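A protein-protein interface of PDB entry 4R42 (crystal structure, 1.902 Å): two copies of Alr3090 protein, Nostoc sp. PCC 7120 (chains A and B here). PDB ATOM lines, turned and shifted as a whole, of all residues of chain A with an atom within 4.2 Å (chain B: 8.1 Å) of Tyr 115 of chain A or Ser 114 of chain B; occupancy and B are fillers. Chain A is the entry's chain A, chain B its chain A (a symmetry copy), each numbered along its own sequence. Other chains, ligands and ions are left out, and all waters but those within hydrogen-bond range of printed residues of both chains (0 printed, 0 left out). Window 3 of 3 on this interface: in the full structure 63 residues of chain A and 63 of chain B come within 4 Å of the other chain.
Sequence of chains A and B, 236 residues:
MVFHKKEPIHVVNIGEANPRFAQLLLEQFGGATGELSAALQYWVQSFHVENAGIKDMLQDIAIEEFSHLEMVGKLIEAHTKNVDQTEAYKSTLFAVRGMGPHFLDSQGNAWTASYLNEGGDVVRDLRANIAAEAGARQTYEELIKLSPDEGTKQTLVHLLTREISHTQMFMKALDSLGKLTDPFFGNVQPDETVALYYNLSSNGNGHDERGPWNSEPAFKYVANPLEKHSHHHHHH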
ATOM      1  N   GLY A  30      -7.142 -15.528   3.237  1.00  0.00           N
ATOM      2  CA  GLY A  30      -5.809 -15.163   2.786  1.00  0.00           C
ATOM      3  C   GLY A  30      -5.304 -15.959   1.596  1.00  0.00           C
ATOM      4  O   GLY A  30      -4.103 -15.996   1.353  1.00  0.00           O
ATOM      5  N   GLY A  31      -6.207 -16.578   0.837  1.00  0.00           N
ATOM      6  CA  GLY A  31      -5.815 -17.329  -0.343  1.00  0.00           C
ATOM      7  C   GLY A  31      -5.969 -16.542  -1.637  1.00  0.00           C
ATOM      8  O   GLY A  31      -6.462 -15.411  -1.623  1.00  0.00           O
ATOM      9  N   ALA A  32      -5.558 -17.151  -2.750  1.00  0.00           N
ATOM     10  CA  ALA A  32      -5.484 -16.466  -4.037  1.00  0.00           C
ATOM     11  C   ALA A  32      -6.855 -15.981  -4.480  1.00  0.00           C
ATOM     12  O   ALA A  32      -6.988 -14.869  -4.971  1.00  0.00           O
ATOM     13  CB  ALA A  32      -4.873 -17.383  -5.111  1.00  0.00           C
ATOM     14  N   SER A  37      -7.971 -10.650  -1.815  1.00  0.00           N
ATOM     15  CA  SER A  37      -7.570 -10.497  -3.207  1.00  0.00           C
ATOM     16  C   SER A  37      -8.588  -9.632  -3.932  1.00  0.00           C
ATOM     17  O   SER A  37      -8.220  -8.722  -4.658  1.00  0.00           O
ATOM     18  CB  SER A  37      -7.433 -11.849  -3.894  1.00  0.00           C
ATOM     19  OG  SER A  37      -6.334 -12.570  -3.364  1.00  0.00           O
ATOM     20  N   ASP A 105      -3.311 -19.054   3.278  1.00  0.00           N
ATOM     21  CA  ASP A 105      -4.305 -19.916   2.657  1.00  0.00           C
ATOM     22  C   ASP A 105      -4.383 -21.252   3.401  1.00  0.00           C
ATOM     23  O   ASP A 105      -3.778 -21.421   4.472  1.00  0.00           O
ATOM     24  CB  ASP A 105      -4.010 -20.104   1.154  1.00  0.00           C
ATOM     25  CG  ASP A 105      -2.740 -20.889   0.870  1.00  0.00           C
ATOM     26  OD1 ASP A 105      -2.176 -21.524   1.786  1.00  0.00           O
ATOM     27  OD2 ASP A 105      -2.310 -20.899  -0.318  1.00  0.00           O
ATOM     28  N   ALA A 110       1.548 -17.603   2.959  1.00  0.00           N
ATOM     29  CA  ALA A 110       1.262 -16.188   3.158  1.00  0.00           C
ATOM     30  C   ALA A 110       0.605 -15.577   1.920  1.00  0.00           C
ATOM     31  O   ALA A 110       1.023 -15.849   0.791  1.00  0.00           O
ATOM     32  CB  ALA A 110       2.562 -15.435   3.511  1.00  0.00           C
ATOM     33  N   TRP A 111      -0.441 -14.776   2.129  1.00  0.00           N
ATOM     34  CA  TRP A 111      -1.055 -14.044   1.034  1.00  0.00           C
ATOM     35  C   TRP A 111       0.017 -13.203   0.375  1.00  0.00           C
ATOM     36  O   TRP A 111       0.870 -12.627   1.059  1.00  0.00           O
ATOM     37  CB  TRP A 111      -2.209 -13.157   1.515  1.00  0.00           C
ATOM     38  CG  TRP A 111      -3.015 -12.553   0.401  1.00  0.00           C
ATOM     39  CD1 TRP A 111      -4.143 -13.068  -0.165  1.00  0.00           C
ATOM     40  CD2 TRP A 111      -2.755 -11.312  -0.276  1.00  0.00           C
ATOM     41  NE1 TRP A 111      -4.608 -12.223  -1.158  1.00  0.00           N
ATOM     42  CE2 TRP A 111      -3.771 -11.140  -1.242  1.00  0.00           C
ATOM     43  CE3 TRP A 111      -1.769 -10.329  -0.152  1.00  0.00           C
ATOM     44  CZ2 TRP A 111      -3.821 -10.025  -2.083  1.00  0.00           C
ATOM     45  CZ3 TRP A 111      -1.824  -9.225  -0.990  1.00  0.00           C
ATOM     46  CH2 TRP A 111      -2.844  -9.082  -1.936  1.00  0.00           C
ATOM     47  N   THR A 112      -0.008 -13.162  -0.949  1.00  0.00           N
ATOM     48  CA  THR A 112       0.921 -12.330  -1.701  1.00  0.00           C
ATOM     49  C   THR A 112       0.186 -11.499  -2.748  1.00  0.00           C
ATOM     50  O   THR A 112      -0.789 -11.963  -3.349  1.00  0.00           O
ATOM     51  CB  THR A 112       2.005 -13.177  -2.405  1.00  0.00           C
ATOM     52  OG1 THR A 112       2.666 -12.367  -3.378  1.00  0.00           O
ATOM     53  CG2 THR A 112       1.393 -14.405  -3.089  1.00  0.00           C
ATOM     54  N   ALA A 113       0.663 -10.278  -2.992  1.00  0.00           N
ATOM     55  CA  ALA A 113       0.051  -9.422  -4.017  1.00  0.00           C
ATOM     56  C   ALA A 113       0.313  -9.949  -5.437  1.00  0.00           C
ATOM     57  O   ALA A 113      -0.255  -9.443  -6.416  1.00  0.00           O
ATOM     58  CB  ALA A 113       0.546  -7.999  -3.897  1.00  0.00           C
ATOM     59  N   SER A 114       1.163 -10.963  -5.548  1.00  0.00           N
ATOM     60  CA  SER A 114       1.312 -11.685  -6.811  1.00  0.00           C
ATOM     61  C   SER A 114      -0.019 -12.306  -7.255  1.00  0.00           C
ATOM     62  O   SER A 114      -0.189 -12.656  -8.417  1.00  0.00           O
ATOM     63  CB  SER A 114       2.387 -12.769  -6.675  1.00  0.00           C
ATOM     64  OG  SER A 114       3.661 -12.174  -6.587  1.00  0.00           O
ATOM     65  N   TYR A 115      -0.956 -12.439  -6.323  1.00  0.00           N
ATOM     66  CA  TYR A 115      -2.300 -12.939  -6.628  1.00  0.00           C
ATOM     67  C   TYR A 115      -3.137 -11.963  -7.452  1.00  0.00           C
ATOM     68  O   TYR A 115      -4.179 -12.348  -8.006  1.00  0.00           O
ATOM     69  CB  TYR A 115      -3.070 -13.246  -5.340  1.00  0.00           C
ATOM     70  CG  TYR A 115      -2.569 -14.421  -4.516  1.00  0.00           C
ATOM     71  CD1 TYR A 115      -1.922 -15.500  -5.104  1.00  0.00           C
ATOM     72  CD2 TYR A 115      -2.780 -14.450  -3.145  1.00  0.00           C
ATOM     73  CE1 TYR A 115      -1.473 -16.581  -4.331  1.00  0.00           C
ATOM     74  CE2 TYR A 115      -2.346 -15.518  -2.365  1.00  0.00           C
ATOM     75  CZ  TYR A 115      -1.701 -16.579  -2.965  1.00  0.00           C
ATOM     76  OH  TYR A 115      -1.289 -17.628  -2.183  1.00  0.00           O
ATOM     77  N   LEU A 116      -2.718 -10.702  -7.498  1.00  0.00           N
ATOM     78  CA  LEU A 116      -3.528  -9.651  -8.112  1.00  0.00           C
ATOM     79  C   LEU A 116      -3.204  -9.506  -9.597  1.00  0.00           C
ATOM     80  O   LEU A 116      -2.060  -9.667 -10.010  1.00  0.00           O
ATOM     81  CB  LEU A 116      -3.308  -8.301  -7.415  1.00  0.00           C
ATOM     82  CG  LEU A 116      -3.522  -8.224  -5.910  1.00  0.00           C
ATOM     83  CD1 LEU A 116      -3.356  -6.788  -5.423  1.00  0.00           C
ATOM     84  CD2 LEU A 116      -4.881  -8.759  -5.530  1.00  0.00           C
ATOM     85  N   ASN A 117      -4.228  -9.209 -10.388  1.00  0.00           N
ATOM     86  CA  ASN A 117      -4.065  -8.900 -11.805  1.00  0.00           C
ATOM     87  C   ASN A 117      -4.702  -7.541 -12.095  1.00  0.00           C
ATOM     88  O   ASN A 117      -5.915  -7.417 -12.083  1.00  0.00           O
ATOM     89  CB  ASN A 117      -4.696 -10.006 -12.645  1.00  0.00           C
ATOM     90  CG  ASN A 117      -4.479  -9.827 -14.147  1.00  0.00           C
ATOM     91  OD1 ASN A 117      -4.006  -8.794 -14.617  1.00  0.00           O
ATOM     92  ND2 ASN A 117      -4.825 -10.854 -14.904  1.00  0.00           N
ATOM     93  N   ALA B  32       4.583 -11.622 -14.461  1.00  0.00           N
ATOM     94  CA  ALA B  32       3.236 -12.111 -14.185  1.00  0.00           C
ATOM     95  C   ALA B  32       2.432 -12.262 -15.466  1.00  0.00           C
ATOM     96  O   ALA B  32       1.726 -13.245 -15.641  1.00  0.00           O
ATOM     97  CB  ALA B  32       2.503 -11.175 -13.207  1.00  0.00           C
ATOM     98  N   SER B  37       3.766 -17.627 -17.960  1.00  0.00           N
ATOM     99  CA  SER B  37       2.485 -17.645 -17.265  1.00  0.00           C
ATOM    100  C   SER B  37       1.415 -18.189 -18.197  1.00  0.00           C
ATOM    101  O   SER B  37       0.626 -19.034 -17.805  1.00  0.00           O
ATOM    102  CB  SER B  37       2.106 -16.255 -16.770  1.00  0.00           C
ATOM    103  OG  SER B  37       2.979 -15.837 -15.735  1.00  0.00           O
ATOM    104  N   GLN B  41      -0.259 -21.824 -17.601  1.00  0.00           N
ATOM    105  CA  GLN B  41      -1.654 -21.745 -17.195  1.00  0.00           C
ATOM    106  C   GLN B  41      -2.526 -22.611 -18.097  1.00  0.00           C
ATOM    107  O   GLN B  41      -3.316 -23.423 -17.618  1.00  0.00           O
ATOM    108  CB  GLN B  41      -2.149 -20.303 -17.221  1.00  0.00           C
ATOM    109  CG  GLN B  41      -3.564 -20.168 -16.692  1.00  0.00           C
ATOM    110  CD  GLN B  41      -3.877 -18.776 -16.224  1.00  0.00           C
ATOM    111  OE1 GLN B  41      -3.217 -18.241 -15.319  1.00  0.00           O
ATOM    112  NE2 GLN B  41      -4.888 -18.174 -16.826  1.00  0.00           N
ATOM    113  N   ALA B 110      11.638 -13.345  -8.934  1.00  0.00           N
ATOM    114  CA  ALA B 110      11.507 -14.696  -9.466  1.00  0.00           C
ATOM    115  C   ALA B 110      10.067 -14.984  -9.891  1.00  0.00           C
ATOM    116  O   ALA B 110       9.121 -14.631  -9.181  1.00  0.00           O
ATOM    117  CB  ALA B 110      11.978 -15.721  -8.413  1.00  0.00           C
ATOM    118  N   TRP B 111       9.899 -15.599 -11.063  1.00  0.00           N
ATOM    119  CA  TRP B 111       8.582 -16.034 -11.499  1.00  0.00           C
ATOM    120  C   TRP B 111       8.019 -16.953 -10.437  1.00  0.00           C
ATOM    121  O   TRP B 111       8.748 -17.773  -9.867  1.00  0.00           O
ATOM    122  CB  TRP B 111       8.637 -16.753 -12.852  1.00  0.00           C
ATOM    123  CG  TRP B 111       7.287 -17.026 -13.450  1.00  0.00           C
ATOM    124  CD1 TRP B 111       6.602 -16.232 -14.322  1.00  0.00           C
ATOM    125  CD2 TRP B 111       6.460 -18.179 -13.222  1.00  0.00           C
ATOM    126  NE1 TRP B 111       5.394 -16.820 -14.655  1.00  0.00           N
ATOM    127  CE2 TRP B 111       5.288 -18.015 -13.992  1.00  0.00           C
ATOM    128  CE3 TRP B 111       6.604 -19.336 -12.449  1.00  0.00           C
ATOM    129  CZ2 TRP B 111       4.263 -18.965 -14.004  1.00  0.00           C
ATOM    130  CZ3 TRP B 111       5.583 -20.275 -12.465  1.00  0.00           C
ATOM    131  CH2 TRP B 111       4.434 -20.085 -13.240  1.00  0.00           C
ATOM    132  N   THR B 112       6.735 -16.794 -10.152  1.00  0.00           N
ATOM    133  CA  THR B 112       6.054 -17.664  -9.203  1.00  0.00           C
ATOM    134  C   THR B 112       4.740 -18.180  -9.782  1.00  0.00           C
ATOM    135  O   THR B 112       4.044 -17.460 -10.506  1.00  0.00           O
ATOM    136  CB  THR B 112       5.763 -16.938  -7.870  1.00  0.00           C
ATOM    137  OG1 THR B 112       4.817 -17.705  -7.122  1.00  0.00           O
ATOM    138  CG2 THR B 112       5.206 -15.531  -8.113  1.00  0.00           C
ATOM    139  N   ALA B 113       4.379 -19.419  -9.446  1.00  0.00           N
ATOM    140  CA  ALA B 113       3.107 -19.986  -9.915  1.00  0.00           C
ATOM    141  C   ALA B 113       1.897 -19.313  -9.247  1.00  0.00           C
ATOM    142  O   ALA B 113       0.744 -19.554  -9.633  1.00  0.00           O
ATOM    143  CB  ALA B 113       3.062 -21.478  -9.678  1.00  0.00           C
ATOM    144  N   SER B 114       2.158 -18.470  -8.255  1.00  0.00           N
ATOM    145  CA  SER B 114       1.111 -17.610  -7.704  1.00  0.00           C
ATOM    146  C   SER B 114       0.521 -16.693  -8.785  1.00  0.00           C
ATOM    147  O   SER B 114      -0.565 -16.151  -8.619  1.00  0.00           O
ATOM    148  CB  SER B 114       1.669 -16.776  -6.545  1.00  0.00           C
ATOM    149  OG  SER B 114       1.910 -17.604  -5.431  1.00  0.00           O
ATOM    150  N   TYR B 115       1.243 -16.527  -9.887  1.00  0.00           N
ATOM    151  CA  TYR B 115       0.761 -15.747 -11.030  1.00  0.00           C
ATOM    152  C   TYR B 115      -0.387 -16.418 -11.782  1.00  0.00           C
ATOM    153  O   TYR B 115      -1.065 -15.769 -12.593  1.00  0.00           O
ATOM    154  CB  TYR B 115       1.893 -15.496 -12.031  1.00  0.00           C
ATOM    155  CG  TYR B 115       3.008 -14.569 -11.573  1.00  0.00           C
ATOM    156  CD1 TYR B 115       2.780 -13.555 -10.653  1.00  0.00           C
ATOM    157  CD2 TYR B 115       4.285 -14.703 -12.098  1.00  0.00           C
ATOM    158  CE1 TYR B 115       3.817 -12.701 -10.248  1.00  0.00           C
ATOM    159  CE2 TYR B 115       5.323 -13.861 -11.711  1.00  0.00           C
ATOM    160  CZ  TYR B 115       5.080 -12.862 -10.792  1.00  0.00           C
ATOM    161  OH  TYR B 115       6.111 -12.035 -10.428  1.00  0.00           O
ATOM    162  N   LEU B 116      -0.577 -17.714 -11.554  1.00  0.00           N
ATOM    163  CA  LEU B 116      -1.532 -18.494 -12.341  1.00  0.00           C
ATOM    164  C   LEU B 116      -2.917 -18.476 -11.696  1.00  0.00           C
ATOM    165  O   LEU B 116      -3.042 -18.472 -10.476  1.00  0.00           O
ATOM    166  CB  LEU B 116      -1.068 -19.949 -12.495  1.00  0.00           C
ATOM    167  CG  LEU B 116       0.318 -20.206 -13.070  1.00  0.00           C
ATOM    168  CD1 LEU B 116       0.553 -21.704 -13.239  1.00  0.00           C
ATOM    169  CD2 LEU B 116       0.497 -19.490 -14.386  1.00  0.00           C
ATOM    170  N   ASN B 117      -3.946 -18.458 -12.534  1.00  0.00           N
ATOM    171  CA  ASN B 117      -5.329 -18.580 -12.086  1.00  0.00           C
ATOM    172  C   ASN B 117      -5.993 -19.739 -12.829  1.00  0.00           C
ATOM    173  O   ASN B 117      -6.260 -19.636 -14.014  1.00  0.00           O
ATOM    174  CB  ASN B 117      -6.062 -17.264 -12.328  1.00  0.00           C
ATOM    175  CG  ASN B 117      -7.492 -17.256 -11.788  1.00  0.00           C
ATOM    176  OD1 ASN B 117      -8.036 -18.278 -11.374  1.00  0.00           O
ATOM    177  ND2 ASN B 117      -8.100 -16.083 -11.788  1.00  0.00           N
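Tyr 115 of chain A touches one residue of chain B. Of the printed residues of chain A, Ser 114 of chain B touches Thr 112 (3.998 Å), Ser 114 (3.5 Å) and Tyr 115 (3.7 Å). Printed residues of chain A within 4 Å of Tyr 115 of chain B: Ser 114 (3.7 Å). Of the printed residues of chain B, Ser 114 of chain A touches Thr 112, Ser 114 and Tyr 115. Asn 117 of chain A touches none of the printed residues of chain B. Ala 110 of chain A touches none of the printed residues of chain B. The nearest printed residue of chain B that does not touch Thr 112 of chain A is Thr 112 of chain B (6.2 Å).
Ser 114 of chain B touches Thr 112 of chain A. Ser 114 of chain A touches Thr 112 of chain B. Ser 114 of chain A touches Ser 114 of chain B (O to O, 3.5 Å). Tyr 115 of chain B touches Ser 114 of chain A (CE1 to OG, 3.7 Å). Ser 114 of chain B touches Tyr 115 of chain A (OG to CE1, 3.7 Å).
Thr 112 of chain A touches Ser 114 of chain B, and with the chains exchanged Ser 114 of chain A touches Thr 112 of chain B. Ser 114 of chain A touches its own counterpart, Ser 114 of chain B. Ser 114 of chain A touches Tyr 115 of chain B, and with the chains exchanged Tyr 115 of chain A touches Ser 114 of chain B. Positions printed for both chains: 32, 37, 110, 111, 112, 113, 114, 115, 116 and 117.
The side-chain hydroxyl (OG1) of Thr 112 of chain A lies within hydrogen-bond range of the backbone NH (N) of Ser 114 of chain A (3.0 Å). The side-chain hydroxyl (OG1) of Thr 112 of chain B lies within hydrogen-bond range of the backbone NH (N) of Ser 114 of chain B (3.0 Å).
Of the 13 printed residues of chain A, 3 touch a printed residue of chain B. Along chain A the printed residues that touch a printed residue of chain B span positions 112 to 115. Of the 11 printed residues of chain B, 3 touch a printed residue of chain A. Among the printed residues, 5 pairs touch across the chains.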
